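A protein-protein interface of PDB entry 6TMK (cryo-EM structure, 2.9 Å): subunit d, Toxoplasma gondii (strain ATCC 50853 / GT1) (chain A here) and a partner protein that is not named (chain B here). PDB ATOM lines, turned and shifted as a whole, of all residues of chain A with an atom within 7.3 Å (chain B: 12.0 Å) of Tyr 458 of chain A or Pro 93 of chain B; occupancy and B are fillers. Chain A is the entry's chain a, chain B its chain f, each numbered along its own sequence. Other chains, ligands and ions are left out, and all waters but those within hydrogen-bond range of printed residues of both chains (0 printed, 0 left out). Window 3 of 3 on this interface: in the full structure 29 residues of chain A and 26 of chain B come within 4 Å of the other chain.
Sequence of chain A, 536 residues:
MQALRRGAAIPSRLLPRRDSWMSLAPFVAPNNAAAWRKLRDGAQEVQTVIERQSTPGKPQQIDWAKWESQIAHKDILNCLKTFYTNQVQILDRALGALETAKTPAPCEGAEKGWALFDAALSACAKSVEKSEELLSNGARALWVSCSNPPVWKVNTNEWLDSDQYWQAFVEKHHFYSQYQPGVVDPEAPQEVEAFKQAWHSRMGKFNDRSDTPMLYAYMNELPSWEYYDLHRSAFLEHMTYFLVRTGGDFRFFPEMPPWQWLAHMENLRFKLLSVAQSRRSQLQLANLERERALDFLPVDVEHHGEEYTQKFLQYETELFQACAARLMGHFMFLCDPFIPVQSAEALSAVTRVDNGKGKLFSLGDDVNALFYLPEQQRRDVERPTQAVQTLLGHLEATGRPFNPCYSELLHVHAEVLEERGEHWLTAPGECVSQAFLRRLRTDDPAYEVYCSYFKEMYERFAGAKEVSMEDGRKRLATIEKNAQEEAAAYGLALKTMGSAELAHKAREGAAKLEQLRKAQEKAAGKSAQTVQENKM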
ATOM      1  N   PHE A 331     -25.599   5.684  -1.593  1.00  0.00           N
ATOM      2  CA  PHE A 331     -25.531   4.319  -2.110  1.00  0.00           C
ATOM      3  C   PHE A 331     -26.350   3.367  -1.247  1.00  0.00           C
ATOM      4  O   PHE A 331     -25.948   2.234  -0.979  1.00  0.00           O
ATOM      5  CB  PHE A 331     -24.083   3.848  -2.220  1.00  0.00           C
ATOM      6  CG  PHE A 331     -23.246   4.693  -3.127  1.00  0.00           C
ATOM      7  CD1 PHE A 331     -23.229   4.462  -4.488  1.00  0.00           C
ATOM      8  CD2 PHE A 331     -22.488   5.730  -2.622  1.00  0.00           C
ATOM      9  CE1 PHE A 331     -22.465   5.241  -5.328  1.00  0.00           C
ATOM     10  CE2 PHE A 331     -21.720   6.512  -3.457  1.00  0.00           C
ATOM     11  CZ  PHE A 331     -21.711   6.268  -4.812  1.00  0.00           C
ATOM     12  N   LEU A 334     -30.906   0.959  -3.723  1.00  0.00           N
ATOM     13  CA  LEU A 334     -31.232  -0.441  -3.990  1.00  0.00           C
ATOM     14  C   LEU A 334     -29.957  -1.254  -3.818  1.00  0.00           C
ATOM     15  O   LEU A 334     -29.251  -1.551  -4.783  1.00  0.00           O
ATOM     16  CB  LEU A 334     -31.830  -0.602  -5.374  1.00  0.00           C
ATOM     17  CG  LEU A 334     -33.304  -0.216  -5.484  1.00  0.00           C
ATOM     18  CD1 LEU A 334     -33.730  -0.198  -6.923  1.00  0.00           C
ATOM     19  CD2 LEU A 334     -34.164  -1.176  -4.700  1.00  0.00           C
ATOM     20  N   ASP A 336     -29.021  -4.790  -2.349  1.00  0.00           N
ATOM     21  CA  ASP A 336     -29.359  -6.110  -1.853  1.00  0.00           C
ATOM     22  C   ASP A 336     -28.369  -7.075  -2.487  1.00  0.00           C
ATOM     23  O   ASP A 336     -27.939  -6.850  -3.624  1.00  0.00           O
ATOM     24  CB  ASP A 336     -30.800  -6.490  -2.238  1.00  0.00           C
ATOM     25  CG  ASP A 336     -31.519  -7.289  -1.163  1.00  0.00           C
ATOM     26  OD1 ASP A 336     -30.975  -7.459  -0.055  1.00  0.00           O
ATOM     27  OD2 ASP A 336     -32.647  -7.755  -1.432  1.00  0.00           O
ATOM     28  N   PHE A 338     -27.098  -6.782   0.402  1.00  0.00           N
ATOM     29  CA  PHE A 338     -26.678  -5.865   1.448  1.00  0.00           C
ATOM     30  C   PHE A 338     -27.883  -5.218   2.121  1.00  0.00           C
ATOM     31  O   PHE A 338     -28.987  -5.167   1.576  1.00  0.00           O
ATOM     32  CB  PHE A 338     -25.766  -4.784   0.875  1.00  0.00           C
ATOM     33  CG  PHE A 338     -24.512  -5.320   0.257  1.00  0.00           C
ATOM     34  CD1 PHE A 338     -23.367  -5.477   1.014  1.00  0.00           C
ATOM     35  CD2 PHE A 338     -24.478  -5.672  -1.077  1.00  0.00           C
ATOM     36  CE1 PHE A 338     -22.213  -5.968   0.450  1.00  0.00           C
ATOM     37  CE2 PHE A 338     -23.325  -6.167  -1.645  1.00  0.00           C
ATOM     38  CZ  PHE A 338     -22.192  -6.317  -0.880  1.00  0.00           C
ATOM     39  N   CYS A 431     -30.992 -10.196  -8.636  1.00  0.00           N
ATOM     40  CA  CYS A 431     -30.940  -9.222  -7.556  1.00  0.00           C
ATOM     41  C   CYS A 431     -31.922  -8.089  -7.823  1.00  0.00           C
ATOM     42  O   CYS A 431     -32.431  -7.915  -8.933  1.00  0.00           O
ATOM     43  CB  CYS A 431     -29.520  -8.671  -7.392  1.00  0.00           C
ATOM     44  SG  CYS A 431     -29.093  -7.350  -8.539  1.00  0.00           S
ATOM     45  N   VAL A 432     -32.181  -7.308  -6.773  1.00  0.00           N
ATOM     46  CA  VAL A 432     -33.219  -6.287  -6.856  1.00  0.00           C
ATOM     47  C   VAL A 432     -32.814  -5.171  -7.803  1.00  0.00           C
ATOM     48  O   VAL A 432     -33.661  -4.603  -8.501  1.00  0.00           O
ATOM     49  CB  VAL A 432     -33.528  -5.744  -5.452  1.00  0.00           C
ATOM     50  CG1 VAL A 432     -34.438  -4.543  -5.540  1.00  0.00           C
ATOM     51  CG2 VAL A 432     -34.155  -6.826  -4.607  1.00  0.00           C
ATOM     52  N   SER A 433     -31.526  -4.834  -7.852  1.00  0.00           N
ATOM     53  CA  SER A 433     -31.064  -3.832  -8.803  1.00  0.00           C
ATOM     54  C   SER A 433     -31.269  -4.302 -10.235  1.00  0.00           C
ATOM     55  O   SER A 433     -31.705  -3.530 -11.099  1.00  0.00           O
ATOM     56  CB  SER A 433     -29.595  -3.513  -8.542  1.00  0.00           C
ATOM     57  OG  SER A 433     -28.817  -4.695  -8.520  1.00  0.00           O
ATOM     58  N   GLN A 434     -30.959  -5.571 -10.506  1.00  0.00           N
ATOM     59  CA  GLN A 434     -31.178  -6.112 -11.839  1.00  0.00           C
ATOM     60  C   GLN A 434     -32.658  -6.130 -12.182  1.00  0.00           C
ATOM     61  O   GLN A 434     -33.042  -5.847 -13.321  1.00  0.00           O
ATOM     62  CB  GLN A 434     -30.593  -7.519 -11.934  1.00  0.00           C
ATOM     63  CG  GLN A 434     -29.084  -7.557 -12.007  1.00  0.00           C
ATOM     64  CD  GLN A 434     -28.555  -7.103 -13.346  1.00  0.00           C
ATOM     65  OE1 GLN A 434     -28.390  -7.903 -14.266  1.00  0.00           O
ATOM     66  NE2 GLN A 434     -28.283  -5.811 -13.463  1.00  0.00           N
ATOM     67  N   ALA A 435     -33.509  -6.433 -11.202  1.00  0.00           N
ATOM     68  CA  ALA A 435     -34.947  -6.415 -11.446  1.00  0.00           C
ATOM     69  C   ALA A 435     -35.431  -5.006 -11.755  1.00  0.00           C
ATOM     70  O   ALA A 435     -36.281  -4.810 -12.632  1.00  0.00           O
ATOM     71  CB  ALA A 435     -35.689  -6.977 -10.241  1.00  0.00           C
ATOM     72  N   LEU A 437     -33.641  -2.509 -13.071  1.00  0.00           N
ATOM     73  CA  LEU A 437     -33.183  -2.137 -14.405  1.00  0.00           C
ATOM     74  C   LEU A 437     -33.929  -2.900 -15.488  1.00  0.00           C
ATOM     75  O   LEU A 437     -34.099  -2.394 -16.603  1.00  0.00           O
ATOM     76  CB  LEU A 437     -31.685  -2.382 -14.531  1.00  0.00           C
ATOM     77  CG  LEU A 437     -30.826  -1.481 -13.657  1.00  0.00           C
ATOM     78  CD1 LEU A 437     -29.443  -2.065 -13.520  1.00  0.00           C
ATOM     79  CD2 LEU A 437     -30.774  -0.090 -14.241  1.00  0.00           C
ATOM     80  N   CYS A 451     -28.756   4.178 -14.526  1.00  0.00           N
ATOM     81  CA  CYS A 451     -27.644   3.358 -14.995  1.00  0.00           C
ATOM     82  C   CYS A 451     -26.315   3.863 -14.444  1.00  0.00           C
ATOM     83  O   CYS A 451     -25.474   3.070 -14.007  1.00  0.00           O
ATOM     84  CB  CYS A 451     -27.622   3.342 -16.520  1.00  0.00           C
ATOM     85  SG  CYS A 451     -28.852   2.260 -17.266  1.00  0.00           S
ATOM     86  N   SER A 452     -26.113   5.182 -14.457  1.00  0.00           N
ATOM     87  CA  SER A 452     -24.945   5.783 -13.823  1.00  0.00           C
ATOM     88  C   SER A 452     -24.832   5.354 -12.368  1.00  0.00           C
ATOM     89  O   SER A 452     -23.771   4.901 -11.913  1.00  0.00           O
ATOM     90  CB  SER A 452     -25.026   7.304 -13.927  1.00  0.00           C
ATOM     91  OG  SER A 452     -25.049   7.715 -15.280  1.00  0.00           O
ATOM     92  N   TYR A 453     -25.919   5.522 -11.614  1.00  0.00           N
ATOM     93  CA  TYR A 453     -25.882   5.200 -10.195  1.00  0.00           C
ATOM     94  C   TYR A 453     -25.509   3.745  -9.980  1.00  0.00           C
ATOM     95  O   TYR A 453     -24.680   3.428  -9.125  1.00  0.00           O
ATOM     96  CB  TYR A 453     -27.229   5.488  -9.546  1.00  0.00           C
ATOM     97  CG  TYR A 453     -27.355   4.851  -8.187  1.00  0.00           C
ATOM     98  CD1 TYR A 453     -26.742   5.407  -7.078  1.00  0.00           C
ATOM     99  CD2 TYR A 453     -28.073   3.681  -8.016  1.00  0.00           C
ATOM    100  CE1 TYR A 453     -26.849   4.821  -5.837  1.00  0.00           C
ATOM    101  CE2 TYR A 453     -28.186   3.087  -6.781  1.00  0.00           C
ATOM    102  CZ  TYR A 453     -27.569   3.657  -5.696  1.00  0.00           C
ATOM    103  OH  TYR A 453     -27.689   3.062  -4.464  1.00  0.00           O
ATOM    104  N   PHE A 454     -26.133   2.838 -10.728  1.00  0.00           N
ATOM    105  CA  PHE A 454     -25.897   1.422 -10.483  1.00  0.00           C
ATOM    106  C   PHE A 454     -24.500   1.012 -10.924  1.00  0.00           C
ATOM    107  O   PHE A 454     -23.882   0.151 -10.291  1.00  0.00           O
ATOM    108  CB  PHE A 454     -26.961   0.587 -11.185  1.00  0.00           C
ATOM    109  CG  PHE A 454     -28.266   0.552 -10.455  1.00  0.00           C
ATOM    110  CD1 PHE A 454     -28.369  -0.081  -9.233  1.00  0.00           C
ATOM    111  CD2 PHE A 454     -29.386   1.162 -10.982  1.00  0.00           C
ATOM    112  CE1 PHE A 454     -29.562  -0.110  -8.555  1.00  0.00           C
ATOM    113  CE2 PHE A 454     -30.582   1.134 -10.307  1.00  0.00           C
ATOM    114  CZ  PHE A 454     -30.668   0.501  -9.090  1.00  0.00           C
ATOM    115  N   LYS A 455     -23.973   1.639 -11.975  1.00  0.00           N
ATOM    116  CA  LYS A 455     -22.583   1.413 -12.357  1.00  0.00           C
ATOM    117  C   LYS A 455     -21.644   1.799 -11.223  1.00  0.00           C
ATOM    118  O   LYS A 455     -20.765   1.019 -10.824  1.00  0.00           O
ATOM    119  CB  LYS A 455     -22.265   2.210 -13.619  1.00  0.00           C
ATOM    120  CG  LYS A 455     -21.233   1.573 -14.518  1.00  0.00           C
ATOM    121  CD  LYS A 455     -20.936   2.466 -15.706  1.00  0.00           C
ATOM    122  CE  LYS A 455     -19.947   1.824 -16.659  1.00  0.00           C
ATOM    123  NZ  LYS A 455     -19.426   2.807 -17.645  1.00  0.00           N
ATOM    124  N   GLU A 456     -21.818   3.011 -10.693  1.00  0.00           N
ATOM    125  CA  GLU A 456     -20.967   3.472  -9.601  1.00  0.00           C
ATOM    126  C   GLU A 456     -21.113   2.575  -8.378  1.00  0.00           C
ATOM    127  O   GLU A 456     -20.120   2.235  -7.721  1.00  0.00           O
ATOM    128  CB  GLU A 456     -21.318   4.917  -9.255  1.00  0.00           C
ATOM    129  CG  GLU A 456     -20.383   5.561  -8.259  1.00  0.00           C
ATOM    130  CD  GLU A 456     -20.595   7.057  -8.154  1.00  0.00           C
ATOM    131  OE1 GLU A 456     -19.654   7.765  -7.738  1.00  0.00           O
ATOM    132  OE2 GLU A 456     -21.703   7.525  -8.490  1.00  0.00           O
ATOM    133  N   MET A 457     -22.341   2.166  -8.071  1.00  0.00           N
ATOM    134  CA  MET A 457     -22.582   1.336  -6.900  1.00  0.00           C
ATOM    135  C   MET A 457     -21.919  -0.023  -7.054  1.00  0.00           C
ATOM    136  O   MET A 457     -21.337  -0.548  -6.101  1.00  0.00           O
ATOM    137  CB  MET A 457     -24.082   1.181  -6.676  1.00  0.00           C
ATOM    138  CG  MET A 457     -24.458   0.690  -5.299  1.00  0.00           C
ATOM    139  SD  MET A 457     -26.182   0.184  -5.204  1.00  0.00           S
ATOM    140  CE  MET A 457     -26.092  -1.411  -6.006  1.00  0.00           C
ATOM    141  N   TYR A 458     -21.995  -0.607  -8.250  1.00  0.00           N
ATOM    142  CA  TYR A 458     -21.359  -1.894  -8.488  1.00  0.00           C
ATOM    143  C   TYR A 458     -19.850  -1.778  -8.342  1.00  0.00           C
ATOM    144  O   TYR A 458     -19.214  -2.594  -7.661  1.00  0.00           O
ATOM    145  CB  TYR A 458     -21.716  -2.401  -9.884  1.00  0.00           C
ATOM    146  CG  TYR A 458     -23.158  -2.815 -10.062  1.00  0.00           C
ATOM    147  CD1 TYR A 458     -23.853  -3.450  -9.047  1.00  0.00           C
ATOM    148  CD2 TYR A 458     -23.819  -2.580 -11.256  1.00  0.00           C
ATOM    149  CE1 TYR A 458     -25.167  -3.827  -9.213  1.00  0.00           C
ATOM    150  CE2 TYR A 458     -25.131  -2.955 -11.431  1.00  0.00           C
ATOM    151  CZ  TYR A 458     -25.800  -3.576 -10.406  1.00  0.00           C
ATOM    152  OH  TYR A 458     -27.107  -3.956 -10.573  1.00  0.00           O
ATOM    153  N   GLU A 459     -19.253  -0.768  -8.978  1.00  0.00           N
ATOM    154  CA  GLU A 459     -17.801  -0.652  -8.931  1.00  0.00           C
ATOM    155  C   GLU A 459     -17.299  -0.248  -7.550  1.00  0.00           C
ATOM    156  O   GLU A 459     -16.115  -0.450  -7.256  1.00  0.00           O
ATOM    157  CB  GLU A 459     -17.306   0.338  -9.988  1.00  0.00           C
ATOM    158  CG  GLU A 459     -17.836   1.751  -9.839  1.00  0.00           C
ATOM    159  CD  GLU A 459     -17.015   2.599  -8.887  1.00  0.00           C
ATOM    160  OE1 GLU A 459     -15.927   2.149  -8.469  1.00  0.00           O
ATOM    161  OE2 GLU A 459     -17.456   3.721  -8.559  1.00  0.00           O
ATOM    162  N   ARG A 460     -18.159   0.309  -6.695  1.00  0.00           N
ATOM    163  CA  ARG A 460     -17.753   0.585  -5.320  1.00  0.00           C
ATOM    164  C   ARG A 460     -17.900  -0.650  -4.438  1.00  0.00           C
ATOM    165  O   ARG A 460     -16.986  -0.997  -3.680  1.00  0.00           O
ATOM    166  CB  ARG A 460     -18.569   1.745  -4.749  1.00  0.00           C
ATOM    167  CG  ARG A 460     -18.239   3.088  -5.369  1.00  0.00           C
ATOM    168  CD  ARG A 460     -16.895   3.623  -4.901  1.00  0.00           C
ATOM    169  NE  ARG A 460     -16.848   3.850  -3.459  1.00  0.00           N
ATOM    170  CZ  ARG A 460     -17.281   4.955  -2.861  1.00  0.00           C
ATOM    171  NH1 ARG A 460     -17.799   5.946  -3.574  1.00  0.00           N
ATOM    172  NH2 ARG A 460     -17.196   5.074  -1.544  1.00  0.00           N
ATOM    173  N   PHE A 461     -19.045  -1.329  -4.526  1.00  0.00           N
ATOM    174  CA  PHE A 461     -19.272  -2.520  -3.721  1.00  0.00           C
ATOM    175  C   PHE A 461     -18.344  -3.661  -4.107  1.00  0.00           C
ATOM    176  O   PHE A 461     -18.123  -4.563  -3.293  1.00  0.00           O
ATOM    177  CB  PHE A 461     -20.725  -2.970  -3.853  1.00  0.00           C
ATOM    178  CG  PHE A 461     -21.631  -2.403  -2.803  1.00  0.00           C
ATOM    179  CD1 PHE A 461     -21.850  -3.086  -1.622  1.00  0.00           C
ATOM    180  CD2 PHE A 461     -22.256  -1.187  -2.992  1.00  0.00           C
ATOM    181  CE1 PHE A 461     -22.681  -2.568  -0.653  1.00  0.00           C
ATOM    182  CE2 PHE A 461     -23.087  -0.665  -2.028  1.00  0.00           C
ATOM    183  CZ  PHE A 461     -23.298  -1.354  -0.857  1.00  0.00           C
ATOM    184  N   ALA A 462     -17.798  -3.646  -5.324  1.00  0.00           N
ATOM    185  CA  ALA A 462     -16.805  -4.652  -5.680  1.00  0.00           C
ATOM    186  C   ALA A 462     -15.576  -4.538  -4.789  1.00  0.00           C
ATOM    187  O   ALA A 462     -15.006  -5.552  -4.370  1.00  0.00           O
ATOM    188  CB  ALA A 462     -16.418  -4.508  -7.150  1.00  0.00           C
ATOM    189  N   GLY A 463     -15.157  -3.312  -4.488  1.00  0.00           N
ATOM    190  CA  GLY A 463     -13.972  -3.052  -3.701  1.00  0.00           C
ATOM    191  C   GLY A 463     -14.231  -2.611  -2.277  1.00  0.00           C
ATOM    192  O   GLY A 463     -13.285  -2.202  -1.594  1.00  0.00           O
ATOM    193  N   ALA A 464     -15.473  -2.671  -1.806  1.00  0.00           N
ATOM    194  CA  ALA A 464     -15.753  -2.323  -0.420  1.00  0.00           C
ATOM    195  C   ALA A 464     -14.983  -3.231   0.531  1.00  0.00           C
ATOM    196  O   ALA A 464     -14.809  -4.426   0.277  1.00  0.00           O
ATOM    197  CB  ALA A 464     -17.251  -2.425  -0.137  1.00  0.00           C
ATOM    198  N   ALA B  88     -28.155  -1.866 -23.548  1.00  0.00           N
ATOM    199  CA  ALA B  88     -27.434  -2.600 -22.523  1.00  0.00           C
ATOM    200  C   ALA B  88     -27.509  -1.885 -21.182  1.00  0.00           C
ATOM    201  O   ALA B  88     -27.602  -0.656 -21.111  1.00  0.00           O
ATOM    202  CB  ALA B  88     -25.973  -2.782 -22.925  1.00  0.00           C
ATOM    203  N   THR B  89     -27.468  -2.669 -20.114  1.00  0.00           N
ATOM    204  CA  THR B  89     -27.462  -2.161 -18.754  1.00  0.00           C
ATOM    205  C   THR B  89     -26.269  -2.732 -18.008  1.00  0.00           C
ATOM    206  O   THR B  89     -25.716  -3.765 -18.399  1.00  0.00           O
ATOM    207  CB  THR B  89     -28.756  -2.535 -18.017  1.00  0.00           C
ATOM    208  OG1 THR B  89     -28.905  -3.959 -17.995  1.00  0.00           O
ATOM    209  CG2 THR B  89     -29.950  -1.919 -18.700  1.00  0.00           C
ATOM    210  N   PRO B  90     -25.847  -2.079 -16.928  1.00  0.00           N
ATOM    211  CA  PRO B  90     -24.680  -2.564 -16.187  1.00  0.00           C
ATOM    212  C   PRO B  90     -24.896  -3.957 -15.618  1.00  0.00           C
ATOM    213  O   PRO B  90     -26.014  -4.353 -15.286  1.00  0.00           O
ATOM    214  CB  PRO B  90     -24.517  -1.528 -15.068  1.00  0.00           C
ATOM    215  CG  PRO B  90     -25.828  -0.815 -15.016  1.00  0.00           C
ATOM    216  CD  PRO B  90     -26.286  -0.774 -16.422  1.00  0.00           C
ATOM    217  N   THR B  91     -23.798  -4.700 -15.511  1.00  0.00           N
ATOM    218  CA  THR B  91     -23.805  -6.041 -14.960  1.00  0.00           C
ATOM    219  C   THR B  91     -23.106  -6.047 -13.605  1.00  0.00           C
ATOM    220  O   THR B  91     -22.114  -5.333 -13.423  1.00  0.00           O
ATOM    221  CB  THR B  91     -23.113  -7.039 -15.894  1.00  0.00           C
ATOM    222  OG1 THR B  91     -23.049  -8.324 -15.266  1.00  0.00           O
ATOM    223  CG2 THR B  91     -21.708  -6.575 -16.240  1.00  0.00           C
ATOM    224  N   PRO B  92     -23.587  -6.823 -12.640  1.00  0.00           N
ATOM    225  CA  PRO B  92     -23.044  -6.735 -11.290  1.00  0.00           C
ATOM    226  C   PRO B  92     -21.818  -7.615 -11.136  1.00  0.00           C
ATOM    227  O   PRO B  92     -21.535  -8.458 -12.001  1.00  0.00           O
ATOM    228  CB  PRO B  92     -24.206  -7.236 -10.427  1.00  0.00           C
ATOM    229  CG  PRO B  92     -24.823  -8.290 -11.276  1.00  0.00           C
ATOM    230  CD  PRO B  92     -24.673  -7.816 -12.714  1.00  0.00           C
ATOM    231  N   PRO B  93     -21.066  -7.455 -10.051  1.00  0.00           N
ATOM    232  CA  PRO B  93     -19.974  -8.386  -9.760  1.00  0.00           C
ATOM    233  C   PRO B  93     -20.501  -9.686  -9.179  1.00  0.00           C
ATOM    234  O   PRO B  93     -21.706  -9.812  -8.913  1.00  0.00           O
ATOM    235  CB  PRO B  93     -19.124  -7.621  -8.737  1.00  0.00           C
ATOM    236  CG  PRO B  93     -20.087  -6.712  -8.072  1.00  0.00           C
ATOM    237  CD  PRO B  93     -21.070  -6.310  -9.127  1.00  0.00           C
ATOM    238  N   PRO B  94     -19.631 -10.678  -8.959  1.00  0.00           N
ATOM    239  CA  PRO B  94     -20.119 -11.994  -8.523  1.00  0.00           C
ATOM    240  C   PRO B  94     -20.361 -12.086  -7.024  1.00  0.00           C
ATOM    241  O   PRO B  94     -20.010 -13.090  -6.396  1.00  0.00           O
ATOM    242  CB  PRO B  94     -18.992 -12.944  -8.962  1.00  0.00           C
ATOM    243  CG  PRO B  94     -18.067 -12.109  -9.823  1.00  0.00           C
ATOM    244  CD  PRO B  94     -18.201 -10.731  -9.287  1.00  0.00           C
ATOM    245  N   VAL B  95     -20.967 -11.052  -6.440  1.00  0.00           N
ATOM    246  CA  VAL B  95     -21.471 -11.104  -5.077  1.00  0.00           C
ATOM    247  C   VAL B  95     -22.980 -10.910  -5.030  1.00  0.00           C
ATOM    248  O   VAL B  95     -23.671 -11.562  -4.240  1.00  0.00           O
ATOM    249  CB  VAL B  95     -20.768 -10.062  -4.180  1.00  0.00           C
ATOM    250  CG1 VAL B  95     -20.944  -8.665  -4.738  1.00  0.00           C
ATOM    251  CG2 VAL B  95     -21.314 -10.132  -2.769  1.00  0.00           C
ATOM    252  N   PHE B  96     -23.509 -10.018  -5.868  1.00  0.00           N
ATOM    253  CA  PHE B  96     -24.953  -9.859  -5.964  1.00  0.00           C
ATOM    254  C   PHE B  96     -25.610 -11.120  -6.502  1.00  0.00           C
ATOM    255  O   PHE B  96     -26.754 -11.427  -6.149  1.00  0.00           O
ATOM    256  CB  PHE B  96     -25.278  -8.667  -6.859  1.00  0.00           C
ATOM    257  CG  PHE B  96     -24.833  -7.349  -6.300  1.00  0.00           C
ATOM    258  CD1 PHE B  96     -25.693  -6.574  -5.549  1.00  0.00           C
ATOM    259  CD2 PHE B  96     -23.554  -6.885  -6.533  1.00  0.00           C
ATOM    260  CE1 PHE B  96     -25.284  -5.362  -5.037  1.00  0.00           C
ATOM    261  CE2 PHE B  96     -23.141  -5.673  -6.024  1.00  0.00           C
ATOM    262  CZ  PHE B  96     -24.008  -4.911  -5.276  1.00  0.00           C
ATOM    263  N   GLU B  97     -24.898 -11.863  -7.350  1.00  0.00           N
ATOM    264  CA  GLU B  97     -25.420 -13.122  -7.866  1.00  0.00           C
ATOM    265  C   GLU B  97     -25.575 -14.164  -6.767  1.00  0.00           C
ATOM    266  O   GLU B  97     -26.439 -15.042  -6.867  1.00  0.00           O
ATOM    267  CB  GLU B  97     -24.501 -13.649  -8.964  1.00  0.00           C
ATOM    268  CG  GLU B  97     -24.334 -12.692 -10.130  1.00  0.00           C
ATOM    269  CD  GLU B  97     -23.385 -13.219 -11.186  1.00  0.00           C
ATOM    270  OE1 GLU B  97     -23.016 -14.409 -11.115  1.00  0.00           O
ATOM    271  OE2 GLU B  97     -23.007 -12.440 -12.086  1.00  0.00           O
ATOM    272  N   ALA B  98     -24.759 -14.089  -5.721  1.00  0.00           N
ATOM    273  CA  ALA B  98     -24.827 -15.049  -4.622  1.00  0.00           C
ATOM    274  C   ALA B  98     -26.060 -14.755  -3.782  1.00  0.00           C
ATOM    275  O   ALA B  98     -26.043 -13.889  -2.904  1.00  0.00           O
ATOM    276  CB  ALA B  98     -23.560 -14.981  -3.779  1.00  0.00           C
ATOM    277  N   VAL B  99     -27.145 -15.479  -4.056  1.00  0.00           N
ATOM    278  CA  VAL B  99     -28.418 -15.294  -3.380  1.00  0.00           C
ATOM    279  C   VAL B  99     -28.971 -16.663  -3.008  1.00  0.00           C
ATOM    280  O   VAL B  99     -28.565 -17.692  -3.550  1.00  0.00           O
ATOM    281  CB  VAL B  99     -29.428 -14.514  -4.246  1.00  0.00           C
ATOM    282  CG1 VAL B  99     -30.610 -14.063  -3.409  1.00  0.00           C
ATOM    283  CG2 VAL B  99     -28.752 -13.320  -4.893  1.00  0.00           C
ATOM    284  N   ALA B 102     -30.186 -19.082  -5.838  1.00  0.00           N
ATOM    285  CA  ALA B 102     -29.289 -19.549  -6.888  1.00  0.00           C
ATOM    286  C   ALA B 102     -28.907 -21.006  -6.661  1.00  0.00           C
ATOM    287  O   ALA B 102     -29.707 -21.796  -6.161  1.00  0.00           O
ATOM    288  CB  ALA B 102     -28.046 -18.678  -6.948  1.00  0.00           C
ATOM    289  N   ARG B 145     -38.331  -8.185 -22.127  1.00  0.00           N
ATOM    290  CA  ARG B 145     -37.336  -8.199 -21.061  1.00  0.00           C
ATOM    291  C   ARG B 145     -37.947  -7.827 -19.717  1.00  0.00           C
ATOM    292  O   ARG B 145     -37.578  -8.398 -18.685  1.00  0.00           O
ATOM    293  CB  ARG B 145     -36.193  -7.250 -21.407  1.00  0.00           C
ATOM    294  CG  ARG B 145     -36.567  -5.786 -21.343  1.00  0.00           C
ATOM    295  CD  ARG B 145     -35.432  -4.927 -21.851  1.00  0.00           C
ATOM    296  NE  ARG B 145     -34.302  -4.930 -20.928  1.00  0.00           N
ATOM    297  CZ  ARG B 145     -33.037  -4.735 -21.285  1.00  0.00           C
ATOM    298  NH1 ARG B 145     -32.083  -4.759 -20.366  1.00  0.00           N
ATOM    299  NH2 ARG B 145     -32.716  -4.510 -22.552  1.00  0.00           N
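NE2 of Gln 434 of chain A lies within hydrogen-bond range of O of Pro 90 of chain B, at 3.3 Å.
The side-chain sulfur of Cys 431 of chain A lies within hydrogen-bond range of the backbone NH of Gln 434 of chain A. The side-chain hydroxyl of Ser 433 of chain A is in hydrogen-bond range of the side-chain hydroxyl of Tyr 458 of chain A.
Among the printed residues, merely in contact across the chains: Asp 336 of chain A with Phe 96 of chain B, Tyr 458 of chain A with Pro 92 of chain B, Tyr 458 of chain A with Phe 96 of chain B, Tyr 458 of chain A with Thr 91 of chain B, Phe 338 of chain A with Phe 96 of chain B, Tyr 458 of chain A with Pro 90 of chain B, Tyr 458 of chain A with Pro 93 of chain B and Gln 434 of chain A with Pro 92 of chain B.
Printed residues of chain B within 4 Å of Tyr 458 of chain A: Pro 90 (3.95 Å), Thr 91 (3.9 Å), Pro 92 (3.7 Å), Pro 93 (3.99 Å) and Phe 96 (3.8 Å). Printed residues of chain A within 4 Å of Pro 93 of chain B: Tyr 458. No residue of chain B comes within 4 Å of Cys 431 of chain A. No residue of chain B comes within 4 Å of Ser 433 of chain A. No residue of chain B comes within 4 Å of Phe 454 of chain A. No residue of chain B comes within 4 Å of Glu 459 of chain A. No residue of chain B comes within 4 Å of Ala 462 of chain A. Of the printed residues of chain A, Pro 92 of chain B touches Gln 434 (3.997 Å) and Tyr 458 (3.7 Å). Printed residues of chain A within 4 Å of Thr 91 of chain B: Tyr 458. Printed residues of chain B within 4 Å of Phe 338 of chain A: Phe 96 (3.9 Å). Cys 451 of chain A touches none of the printed residues of chain B. The nearest printed residue of chain B that does not touch Gln 434 of chain A is Thr 91 of chain B (4.7 Å).
Hydrophobic or aromatic side chains of chain A that line the printed part of chain B: Phe 338 and Tyr 458. Along chain A the printed residues that touch a printed residue of chain B span positions 336 to 458. Of the 14 printed residues of chain B, 5 touch a printed residue of chain A. Hydrophobic or aromatic side chains of chain B within 4 Å of the printed part of chain A: Pro 90, Pro 92, Pro 93 and Phe 96. Among the printed residues, 9 pairs touch across the chains.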
